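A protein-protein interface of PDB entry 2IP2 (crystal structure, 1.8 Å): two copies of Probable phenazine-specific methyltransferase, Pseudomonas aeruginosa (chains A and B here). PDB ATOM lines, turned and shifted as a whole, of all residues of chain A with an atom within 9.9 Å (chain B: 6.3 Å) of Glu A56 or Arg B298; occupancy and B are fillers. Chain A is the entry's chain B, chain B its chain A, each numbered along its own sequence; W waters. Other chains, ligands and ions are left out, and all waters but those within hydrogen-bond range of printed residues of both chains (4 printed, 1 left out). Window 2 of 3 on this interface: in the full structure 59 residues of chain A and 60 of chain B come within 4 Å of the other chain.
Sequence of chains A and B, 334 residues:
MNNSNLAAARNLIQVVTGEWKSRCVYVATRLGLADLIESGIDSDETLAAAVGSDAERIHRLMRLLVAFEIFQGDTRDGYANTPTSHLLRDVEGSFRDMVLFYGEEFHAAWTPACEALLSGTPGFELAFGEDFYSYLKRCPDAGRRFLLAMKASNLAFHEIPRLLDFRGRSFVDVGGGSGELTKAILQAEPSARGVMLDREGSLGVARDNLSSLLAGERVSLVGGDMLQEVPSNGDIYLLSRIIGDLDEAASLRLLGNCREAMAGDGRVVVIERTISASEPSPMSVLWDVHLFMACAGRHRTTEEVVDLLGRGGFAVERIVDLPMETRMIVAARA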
ATOM      1  N   SER A  43       1.952  14.376 -30.298  1.00  0.00           N
ATOM      2  CA  SER A  43       2.915  15.366 -29.781  1.00  0.00           C
ATOM      3  C   SER A  43       2.339  16.778 -29.898  1.00  0.00           C
ATOM      4  O   SER A  43       1.399  17.002 -30.653  1.00  0.00           O
ATOM      5  CB  SER A  43       4.280  15.283 -30.505  1.00  0.00           C
ATOM      6  OG  SER A  43       4.199  15.880 -31.794  1.00  0.00           O
ATOM      7  N   ASP A  44       2.938  17.739 -29.198  1.00  0.00           N
ATOM      8  CA  ASP A  44       2.465  19.148 -29.347  1.00  0.00           C
ATOM      9  C   ASP A  44       2.509  19.590 -30.813  1.00  0.00           C
ATOM     10  O   ASP A  44       1.541  20.176 -31.336  1.00  0.00           O
ATOM     11  CB  ASP A  44       3.292  20.098 -28.486  1.00  0.00           C
ATOM     12  CG  ASP A  44       3.101  19.840 -26.998  1.00  0.00           C
ATOM     13  OD1 ASP A  44       2.010  19.372 -26.604  1.00  0.00           O
ATOM     14  OD2 ASP A  44       4.041  20.097 -26.215  1.00  0.00           O
ATOM     15  N   GLU A  45       3.642  19.289 -31.480  1.00  0.00           N
ATOM     16  CA  GLU A  45       3.863  19.729 -32.852  1.00  0.00           C
ATOM     17  C   GLU A  45       2.890  19.131 -33.833  1.00  0.00           C
ATOM     18  O   GLU A  45       2.330  19.860 -34.667  1.00  0.00           O
ATOM     19  CB  GLU A  45       5.322  19.431 -33.344  1.00  0.00           C
ATOM     20  CG  GLU A  45       6.388  20.303 -32.671  1.00  0.00           C
ATOM     21  CD  GLU A  45       6.614  19.934 -31.196  1.00  0.00           C
ATOM     22  OE1 GLU A  45       6.326  18.753 -30.802  1.00  0.00           O
ATOM     23  OE2 GLU A  45       7.049  20.849 -30.415  1.00  0.00           O
ATOM     24  N   THR A  46       2.692  17.815 -33.760  1.00  0.00           N
ATOM     25  CA  THR A  46       1.824  17.133 -34.729  1.00  0.00           C
ATOM     26  C   THR A  46       0.361  17.490 -34.528  1.00  0.00           C
ATOM     27  O   THR A  46      -0.372  17.668 -35.492  1.00  0.00           O
ATOM     28  CB  THR A  46       2.068  15.580 -34.824  1.00  0.00           C
ATOM     29  OG1 THR A  46       1.854  14.950 -33.542  1.00  0.00           O
ATOM     30  CG2 THR A  46       3.585  15.302 -35.283  1.00  0.00           C
ATOM     31  N   LEU A  47      -0.017  17.645 -33.258  1.00  0.00           N
ATOM     32  CA  LEU A  47      -1.381  18.074 -32.891  1.00  0.00           C
ATOM     33  C   LEU A  47      -1.629  19.513 -33.417  1.00  0.00           C
ATOM     34  O   LEU A  47      -2.636  19.785 -34.063  1.00  0.00           O
ATOM     35  CB  LEU A  47      -1.574  17.962 -31.354  1.00  0.00           C
ATOM     36  CG  LEU A  47      -1.902  16.524 -30.887  1.00  0.00           C
ATOM     37  CD1 LEU A  47      -1.850  16.460 -29.285  1.00  0.00           C
ATOM     38  CD2 LEU A  47      -3.229  15.981 -31.481  1.00  0.00           C
ATOM     39  N   ALA A  48      -0.668  20.398 -33.210  1.00  0.00           N
ATOM     40  CA  ALA A  48      -0.771  21.790 -33.656  1.00  0.00           C
ATOM     41  C   ALA A  48      -0.864  21.844 -35.156  1.00  0.00           C
ATOM     42  O   ALA A  48      -1.668  22.579 -35.711  1.00  0.00           O
ATOM     43  CB  ALA A  48       0.412  22.598 -33.175  1.00  0.00           C
ATOM     44  N   ALA A  49      -0.052  21.027 -35.834  1.00  0.00           N
ATOM     45  CA  ALA A  49      -0.125  20.929 -37.292  1.00  0.00           C
ATOM     46  C   ALA A  49      -1.498  20.458 -37.791  1.00  0.00           C
ATOM     47  O   ALA A  49      -2.085  21.033 -38.702  1.00  0.00           O
ATOM     48  CB  ALA A  49       1.027  20.007 -37.806  1.00  0.00           C
ATOM     49  N   SER A  53      -3.031  25.071 -34.967  1.00  0.00           N
ATOM     50  CA  SER A  53      -2.652  25.902 -33.824  1.00  0.00           C
ATOM     51  C   SER A  53      -1.144  26.003 -33.848  1.00  0.00           C
ATOM     52  O   SER A  53      -0.514  25.741 -34.866  1.00  0.00           O
ATOM     53  CB  SER A  53      -3.195  25.280 -32.497  1.00  0.00           C
ATOM     54  OG  SER A  53      -2.968  26.100 -31.348  1.00  0.00           O
ATOM     55  N   ASP A  54      -0.580  26.372 -32.718  1.00  0.00           N
ATOM     56  CA  ASP A  54       0.830  26.495 -32.503  1.00  0.00           C
ATOM     57  C   ASP A  54       1.200  25.487 -31.422  1.00  0.00           C
ATOM     58  O   ASP A  54       0.413  25.224 -30.491  1.00  0.00           O
ATOM     59  CB  ASP A  54       1.098  27.916 -32.022  1.00  0.00           C
ATOM     60  CG  ASP A  54       2.454  28.100 -31.570  1.00  0.00           C
ATOM     61  OD1 ASP A  54       3.332  28.184 -32.475  1.00  0.00           O
ATOM     62  OD2 ASP A  54       2.641  28.131 -30.320  1.00  0.00           O
ATOM     63  N   ALA A  55       2.414  24.950 -31.510  1.00  0.00           N
ATOM     64  CA  ALA A  55       2.878  23.928 -30.553  1.00  0.00           C
ATOM     65  C   ALA A  55       2.836  24.401 -29.068  1.00  0.00           C
ATOM     66  O   ALA A  55       2.478  23.621 -28.198  1.00  0.00           O
ATOM     67  CB  ALA A  55       4.282  23.437 -30.929  1.00  0.00           C
ATOM     68  N   GLU A  56       3.148  25.671 -28.805  1.00  0.00           N
ATOM     69  CA  GLU A  56       3.188  26.159 -27.403  1.00  0.00           C
ATOM     70  C   GLU A  56       1.754  26.233 -26.840  1.00  0.00           C
ATOM     71  O   GLU A  56       1.519  25.934 -25.664  1.00  0.00           O
ATOM     72  CB  GLU A  56       3.924  27.511 -27.249  1.00  0.00           C
ATOM     73  CG  GLU A  56       4.185  27.960 -25.722  1.00  0.00           C
ATOM     74  CD  GLU A  56       4.135  29.517 -25.456  1.00  0.00           C
ATOM     75  OE1 GLU A  56       3.965  30.310 -26.443  1.00  0.00           O
ATOM     76  OE2 GLU A  56       4.253  29.958 -24.261  1.00  0.00           O
ATOM     77  N   ARG A  57       0.801  26.596 -27.670  1.00  0.00           N
ATOM     78  CA  ARG A  57      -0.593  26.740 -27.170  1.00  0.00           C
ATOM     79  C   ARG A  57      -1.163  25.374 -26.958  1.00  0.00           C
ATOM     80  O   ARG A  57      -1.871  25.114 -25.982  1.00  0.00           O
ATOM     81  CB  ARG A  57      -1.444  27.557 -28.126  1.00  0.00           C
ATOM     82  CG  ARG A  57      -1.129  29.063 -28.079  1.00  0.00           C
ATOM     83  CD  ARG A  57      -2.156  29.915 -28.810  1.00  0.00           C
ATOM     84  NE  ARG A  57      -2.264  29.630 -30.247  1.00  0.00           N
ATOM     85  CZ  ARG A  57      -1.427  30.082 -31.190  1.00  0.00           C
ATOM     86  NH1 ARG A  57      -0.373  30.848 -30.867  1.00  0.00           N
ATOM     87  NH2 ARG A  57      -1.666  29.803 -32.458  1.00  0.00           N
ATOM     88  N   ILE A  58      -0.845  24.464 -27.862  1.00  0.00           N
ATOM     89  CA  ILE A  58      -1.288  23.093 -27.639  1.00  0.00           C
ATOM     90  C   ILE A  58      -0.665  22.550 -26.359  1.00  0.00           C
ATOM     91  O   ILE A  58      -1.332  21.847 -25.576  1.00  0.00           O
ATOM     92  CB  ILE A  58      -0.972  22.182 -28.865  1.00  0.00           C
ATOM     93  CG1 ILE A  58      -1.792  22.647 -30.084  1.00  0.00           C
ATOM     94  CG2 ILE A  58      -1.198  20.643 -28.501  1.00  0.00           C
ATOM     95  CD1 ILE A  58      -3.276  22.320 -29.970  1.00  0.00           C
ATOM     96  N   HIS A  59       0.632  22.825 -26.174  1.00  0.00           N
ATOM     97  CA  HIS A  59       1.340  22.341 -25.001  1.00  0.00           C
ATOM     98  C   HIS A  59       0.612  22.762 -23.723  1.00  0.00           C
ATOM     99  O   HIS A  59       0.411  21.944 -22.790  1.00  0.00           O
ATOM    100  CB  HIS A  59       2.769  22.903 -24.944  1.00  0.00           C
ATOM    101  CG  HIS A  59       3.538  22.399 -23.769  1.00  0.00           C
ATOM    102  ND1 HIS A  59       4.072  21.125 -23.731  1.00  0.00           N
ATOM    103  CD2 HIS A  59       3.796  22.957 -22.561  1.00  0.00           C
ATOM    104  CE1 HIS A  59       4.662  20.936 -22.562  1.00  0.00           C
ATOM    105  NE2 HIS A  59       4.503  22.026 -21.830  1.00  0.00           N
ATOM    106  N   ARG A  60       0.220  24.042 -23.693  1.00  0.00           N
ATOM    107  CA  ARG A  60      -0.440  24.600 -22.511  1.00  0.00           C
ATOM    108  C   ARG A  60      -1.857  24.036 -22.278  1.00  0.00           C
ATOM    109  O   ARG A  60      -2.276  23.774 -21.143  1.00  0.00           O
ATOM    110  CB  ARG A  60      -0.432  26.115 -22.611  1.00  0.00           C
ATOM    111  CG  ARG A  60       0.959  26.695 -22.573  1.00  0.00           C
ATOM    112  CD  ARG A  60       0.976  28.189 -22.993  1.00  0.00           C
ATOM    113  NE  ARG A  60       0.377  29.080 -21.968  1.00  0.00           N
ATOM    114  CZ  ARG A  60       0.333  30.411 -22.097  1.00  0.00           C
ATOM    115  NH1 ARG A  60       0.774  30.958 -23.216  1.00  0.00           N
ATOM    116  NH2 ARG A  60      -0.158  31.188 -21.126  1.00  0.00           N
ATOM    117  N   LEU A  61      -2.582  23.842 -23.363  1.00  0.00           N
ATOM    118  CA  LEU A  61      -3.928  23.252 -23.231  1.00  0.00           C
ATOM    119  C   LEU A  61      -3.817  21.810 -22.736  1.00  0.00           C
ATOM    120  O   LEU A  61      -4.571  21.362 -21.875  1.00  0.00           O
ATOM    121  CB  LEU A  61      -4.640  23.330 -24.562  1.00  0.00           C
ATOM    122  CG  LEU A  61      -5.951  22.532 -24.662  1.00  0.00           C
ATOM    123  CD1 LEU A  61      -6.905  23.088 -23.616  1.00  0.00           C
ATOM    124  CD2 LEU A  61      -6.514  22.672 -26.100  1.00  0.00           C
ATOM    125  N   MET A  62      -2.847  21.086 -23.315  1.00  0.00           N
ATOM    126  CA  MET A  62      -2.614  19.690 -22.921  1.00  0.00           C
ATOM    127  C   MET A  62      -2.106  19.527 -21.494  1.00  0.00           C
ATOM    128  O   MET A  62      -2.566  18.631 -20.789  1.00  0.00           O
ATOM    129  CB  MET A  62      -1.678  19.000 -23.903  1.00  0.00           C
ATOM    130  CG  MET A  62      -2.323  18.740 -25.272  1.00  0.00           C
ATOM    131  SD  MET A  62      -3.845  17.784 -25.337  1.00  0.00           S
ATOM    132  CE  MET A  62      -3.406  16.226 -24.590  1.00  0.00           C
ATOM    133  N   ARG A  63      -1.150  20.364 -21.085  1.00  0.00           N
ATOM    134  CA  ARG A  63      -0.696  20.404 -19.708  1.00  0.00           C
ATOM    135  C   ARG A  63      -1.874  20.540 -18.754  1.00  0.00           C
ATOM    136  O   ARG A  63      -1.941  19.828 -17.746  1.00  0.00           O
ATOM    137  CB  ARG A  63       0.252  21.588 -19.493  1.00  0.00           C
ATOM    138  CG  ARG A  63       1.015  21.503 -18.203  1.00  0.00           C
ATOM    139  CD  ARG A  63       2.156  22.555 -18.136  1.00  0.00           C
ATOM    140  NE  ARG A  63       1.790  23.903 -18.593  1.00  0.00           N
ATOM    141  CZ  ARG A  63       2.644  24.931 -18.611  1.00  0.00           C
ATOM    142  NH1 ARG A  63       3.915  24.763 -18.210  1.00  0.00           N
ATOM    143  NH2 ARG A  63       2.261  26.131 -19.012  1.00  0.00           N
ATOM    144  N   LEU A  64      -2.759  21.491 -19.039  1.00  0.00           N
ATOM    145  CA  LEU A  64      -3.972  21.671 -18.183  1.00  0.00           C
ATOM    146  C   LEU A  64      -4.814  20.369 -18.119  1.00  0.00           C
ATOM    147  O   LEU A  64      -5.168  19.846 -17.035  1.00  0.00           O
ATOM    148  CB  LEU A  64      -4.846  22.849 -18.639  1.00  0.00           C
ATOM    149  CG  LEU A  64      -6.099  22.878 -17.722  1.00  0.00           C
ATOM    150  CD1 LEU A  64      -5.789  23.422 -16.351  1.00  0.00           C
ATOM    151  CD2 LEU A  64      -7.261  23.624 -18.317  1.00  0.00           C
ATOM    152  N   THR A  75       4.408  15.253 -24.237  1.00  0.00           N
ATOM    153  CA  THR A  75       4.654  15.479 -25.659  1.00  0.00           C
ATOM    154  C   THR A  75       5.808  14.604 -26.164  1.00  0.00           C
ATOM    155  O   THR A  75       5.824  14.198 -27.325  1.00  0.00           O
ATOM    156  CB  THR A  75       4.937  16.964 -25.924  1.00  0.00           C
ATOM    157  OG1 THR A  75       4.952  17.207 -27.323  1.00  0.00           O
ATOM    158  CG2 THR A  75       6.293  17.398 -25.319  1.00  0.00           C
ATOM    159  N   TYR A  79       1.163  11.742 -25.958  1.00  0.00           N
ATOM    160  CA  TYR A  79      -0.081  11.784 -25.181  1.00  0.00           C
ATOM    161  C   TYR A  79      -0.902  10.539 -25.470  1.00  0.00           C
ATOM    162  O   TYR A  79      -0.754   9.908 -26.538  1.00  0.00           O
ATOM    163  CB  TYR A  79      -0.899  13.030 -25.537  1.00  0.00           C
ATOM    164  CG  TYR A  79      -0.214  14.349 -25.252  1.00  0.00           C
ATOM    165  CD1 TYR A  79      -0.076  14.815 -23.932  1.00  0.00           C
ATOM    166  CD2 TYR A  79       0.263  15.137 -26.297  1.00  0.00           C
ATOM    167  CE1 TYR A  79       0.520  16.021 -23.656  1.00  0.00           C
ATOM    168  CE2 TYR A  79       0.876  16.364 -26.046  1.00  0.00           C
ATOM    169  CZ  TYR A  79       0.986  16.798 -24.721  1.00  0.00           C
ATOM    170  OH  TYR A  79       1.597  17.989 -24.466  1.00  0.00           O
ATOM    171  N   GLY B 244       7.458  38.040 -15.076  1.00  0.00           N
ATOM    172  CA  GLY B 244       6.625  37.271 -16.027  1.00  0.00           C
ATOM    173  C   GLY B 244       6.463  37.942 -17.379  1.00  0.00           C
ATOM    174  O   GLY B 244       6.326  37.286 -18.422  1.00  0.00           O
ATOM    175  N   ASP B 245       6.500  39.266 -17.375  1.00  0.00           N
ATOM    176  CA  ASP B 245       6.222  39.987 -18.584  1.00  0.00           C
ATOM    177  C   ASP B 245       7.487  40.361 -19.362  1.00  0.00           C
ATOM    178  O   ASP B 245       7.381  40.922 -20.465  1.00  0.00           O
ATOM    179  CB  ASP B 245       5.416  41.252 -18.264  1.00  0.00           C
ATOM    180  CG  ASP B 245       4.711  41.831 -19.488  1.00  0.00           C
ATOM    181  OD1 ASP B 245       4.646  41.149 -20.540  1.00  0.00           O
ATOM    182  OD2 ASP B 245       4.218  42.976 -19.391  1.00  0.00           O
ATOM    183  N   ASP B 288      -2.565  29.380 -15.881  1.00  0.00           N
ATOM    184  CA  ASP B 288      -1.717  29.640 -17.050  1.00  0.00           C
ATOM    185  C   ASP B 288      -2.511  29.806 -18.347  1.00  0.00           C
ATOM    186  O   ASP B 288      -2.234  30.725 -19.130  1.00  0.00           O
ATOM    187  CB  ASP B 288      -0.725  28.513 -17.199  1.00  0.00           C
ATOM    188  CG  ASP B 288       0.156  28.673 -18.459  1.00  0.00           C
ATOM    189  OD1 ASP B 288       0.969  29.613 -18.455  1.00  0.00           O
ATOM    190  OD2 ASP B 288       0.040  27.834 -19.408  1.00  0.00           O
ATOM    191  N   LEU B 291      -4.314  33.072 -18.294  1.00  0.00           N
ATOM    192  CA  LEU B 291      -3.427  34.213 -18.612  1.00  0.00           C
ATOM    193  C   LEU B 291      -3.306  34.449 -20.123  1.00  0.00           C
ATOM    194  O   LEU B 291      -3.326  35.604 -20.588  1.00  0.00           O
ATOM    195  CB  LEU B 291      -2.047  34.031 -17.937  1.00  0.00           C
ATOM    196  CG  LEU B 291      -1.076  35.218 -17.963  1.00  0.00           C
ATOM    197  CD1 LEU B 291      -1.795  36.515 -17.593  1.00  0.00           C
ATOM    198  CD2 LEU B 291       0.032  34.988 -16.966  1.00  0.00           C
ATOM    199  N   PHE B 292      -3.204  33.358 -20.895  1.00  0.00           N
ATOM    200  CA  PHE B 292      -3.284  33.442 -22.318  1.00  0.00           C
ATOM    201  C   PHE B 292      -4.653  34.009 -22.759  1.00  0.00           C
ATOM    202  O   PHE B 292      -4.727  34.936 -23.584  1.00  0.00           O
ATOM    203  CB  PHE B 292      -3.058  32.066 -23.013  1.00  0.00           C
ATOM    204  CG  PHE B 292      -3.483  32.106 -24.454  1.00  0.00           C
ATOM    205  CD1 PHE B 292      -2.681  32.775 -25.402  1.00  0.00           C
ATOM    206  CD2 PHE B 292      -4.763  31.606 -24.844  1.00  0.00           C
ATOM    207  CE1 PHE B 292      -3.135  32.913 -26.729  1.00  0.00           C
ATOM    208  CE2 PHE B 292      -5.215  31.708 -26.146  1.00  0.00           C
ATOM    209  CZ  PHE B 292      -4.396  32.377 -27.114  1.00  0.00           C
ATOM    210  N   ALA B 296      -2.699  37.064 -23.458  1.00  0.00           N
ATOM    211  CA  ALA B 296      -1.539  36.398 -24.112  1.00  0.00           C
ATOM    212  C   ALA B 296      -0.308  36.398 -23.211  1.00  0.00           C
ATOM    213  O   ALA B 296       0.827  36.382 -23.699  1.00  0.00           O
ATOM    214  CB  ALA B 296      -1.181  37.091 -25.508  1.00  0.00           C
ATOM    215  N   GLY B 297      -0.501  36.421 -21.913  1.00  0.00           N
ATOM    216  CA  GLY B 297       0.635  36.274 -21.036  1.00  0.00           C
ATOM    217  C   GLY B 297       0.933  34.801 -20.889  1.00  0.00           C
ATOM    218  O   GLY B 297       0.172  33.955 -21.400  1.00  0.00           O
ATOM    219  N   ARG B 298       2.020  34.492 -20.184  1.00  0.00           N
ATOM    220  CA  ARG B 298       2.268  33.116 -19.734  1.00  0.00           C
ATOM    221  C   ARG B 298       3.085  33.071 -18.438  1.00  0.00           C
ATOM    222  O   ARG B 298       3.752  34.039 -18.105  1.00  0.00           O
ATOM    223  CB  ARG B 298       2.966  32.269 -20.808  1.00  0.00           C
ATOM    224  CG  ARG B 298       4.450  32.558 -21.053  1.00  0.00           C
ATOM    225  CD  ARG B 298       4.652  33.685 -22.065  1.00  0.00           C
ATOM    226  NE  ARG B 298       3.692  33.690 -23.189  1.00  0.00           N
ATOM    227  CZ  ARG B 298       3.927  33.198 -24.413  1.00  0.00           C
ATOM    228  NH1 ARG B 298       5.093  32.634 -24.715  1.00  0.00           N
ATOM    229  NH2 ARG B 298       2.986  33.267 -25.351  1.00  0.00           N
ATOM    230  N   HIS B 299       3.019  31.949 -17.726  1.00  0.00           N
ATOM    231  CA  HIS B 299       3.829  31.758 -16.524  1.00  0.00           C
ATOM    232  C   HIS B 299       5.140  31.019 -16.863  1.00  0.00           C
ATOM    233  O   HIS B 299       5.211  30.238 -17.825  1.00  0.00           O
ATOM    234  CB  HIS B 299       3.010  31.063 -15.415  1.00  0.00           C
ATOM    235  CG  HIS B 299       1.842  31.873 -14.909  1.00  0.00           C
ATOM    236  ND1 HIS B 299       1.991  33.086 -14.274  1.00  0.00           N
ATOM    237  CD2 HIS B 299       0.512  31.622 -14.907  1.00  0.00           C
ATOM    238  CE1 HIS B 299       0.809  33.564 -13.930  1.00  0.00           C
ATOM    239  NE2 HIS B 299      -0.108  32.686 -14.289  1.00  0.00           N
ATOM    240  N   ARG B 300       6.209  31.309 -16.112  1.00  0.00           N
ATOM    241  CA  ARG B 300       7.433  30.526 -16.194  1.00  0.00           C
ATOM    242  C   ARG B 300       7.378  29.317 -15.284  1.00  0.00           C
ATOM    243  O   ARG B 300       6.642  29.275 -14.320  1.00  0.00           O
ATOM    244  CB  ARG B 300       8.617  31.381 -15.769  1.00  0.00           C
ATOM    245  CG  ARG B 300       9.145  32.356 -16.852  1.00  0.00           C
ATOM    246  CD  ARG B 300      10.468  32.918 -16.390  1.00  0.00           C
ATOM    247  NE  ARG B 300      11.168  33.683 -17.424  1.00  0.00           N
ATOM    248  CZ  ARG B 300      10.966  34.980 -17.640  1.00  0.00           C
ATOM    249  NH1 ARG B 300      10.058  35.646 -16.916  1.00  0.00           N
ATOM    250  NH2 ARG B 300      11.663  35.616 -18.575  1.00  0.00           N
HETATM  251  O   HOH W   1       0.679  33.478 -24.500  1.00  0.00           O
HETATM  252  O   HOH W   2       5.195  27.298 -17.888  1.00  0.00           O
HETATM  253  O   HOH W   3      -0.734  25.185 -18.999  1.00  0.00           O
HETATM  254  O   HOH W   4       3.127  29.134 -19.866  1.00  0.00           O
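The guanidinium group (NH2) of Arg A60 is in hydrogen-bond range of the backbone carbonyl oxygen (O) of Gly B297 (2.8 Å).
OD2 of Asp B288 is in salt-bridge range of NH2 of Arg A63.
The side-chain carboxylate (OE2) of Glu A56 lies within salt-bridge range of the guanidinium group (NH1) of Arg B298, at 2.8 Å.
The side-chain carboxylate of Asp B288 lies within salt-bridge range of the guanidinium group of Arg A60 (2.9 Å).
The backbone NH (N) of Phe B292 is in hydrogen-bond range of the backbone carbonyl oxygen (O) of Gly B297, 3.5 Å away.
OD2 of Asp A54 sits at hydrogen-bond distance from N of Glu A56, at 2.9 Å.
The backbone NH of Gly B297 is in hydrogen-bond range of the backbone carbonyl oxygen of Leu B291 (3.2 Å).
The side-chain carboxylate of Glu A56 lies within salt-bridge range of the guanidinium group of Arg A60 (3.8 Å).
N of His B299 sits at hydrogen-bond distance from OD1 of Asp B288 (3.2 Å).
Arg A57 touches Phe B292.
NH2 of Arg A60 touches CB of Phe B292 (3.6 Å).
NH2 of Arg A60 touches CB of Arg B298, 3.3 Å away.
Of chain B, only Arg B298 (2.8 Å) comes within 4 Å of Glu A56.
Of chain A, only Glu A56 and Arg A60 come within 4 Å of Arg B298.
Gly B297 touches one residue of chain A.
No residue of chain A comes within 4 Å of His B299.
Of the printed residues of chain A, Phe B292 touches Arg A57 (3.7 Å) and Arg A60 (3.6 Å).
Printed residues of chain A within 4 Å of Asp B288: Arg A60 (2.9 Å) and Arg A63 (2.8 Å).
Ala A49 touches none of the printed residues of chain B.
Of the 21 printed residues of chain A, 4 touch a printed residue of chain B.
No position is printed for both chains.
Of the 7 pairs that touch across the chains among the printed residues, none has its exchanged pair printed and touching as well.
Water W1 lies within hydrogen-bond range of the guanidinium group of Arg B298 (2.5 Å), the guanidinium group of Arg A60 (2.8 Å), the backbone carbonyl oxygen of Ala B296 (3.0 Å) and the backbone carbonyl oxygen of Gly B297 (3.2 Å).
Water W4 lies within hydrogen-bond range of the side-chain carboxylate (OD1) of Asp B288 (2.6 Å), the backbone carbonyl oxygen (O) of His B299 (3.1 Å), the guanidinium group (NH2) of Arg A63 (3.2 Å) and the guanidinium group (NE) of Arg A60 (3.5 Å).
Water W3 lies within hydrogen-bond range of OD2 of Asp B288 (2.8 Å), NE of Arg A63 (2.9 Å) and O of Arg A60 (3.0 Å).
Water W2 lies within hydrogen-bond range of NH1 of Arg A63 (2.9 Å) and O of His B299 (2.9 Å).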
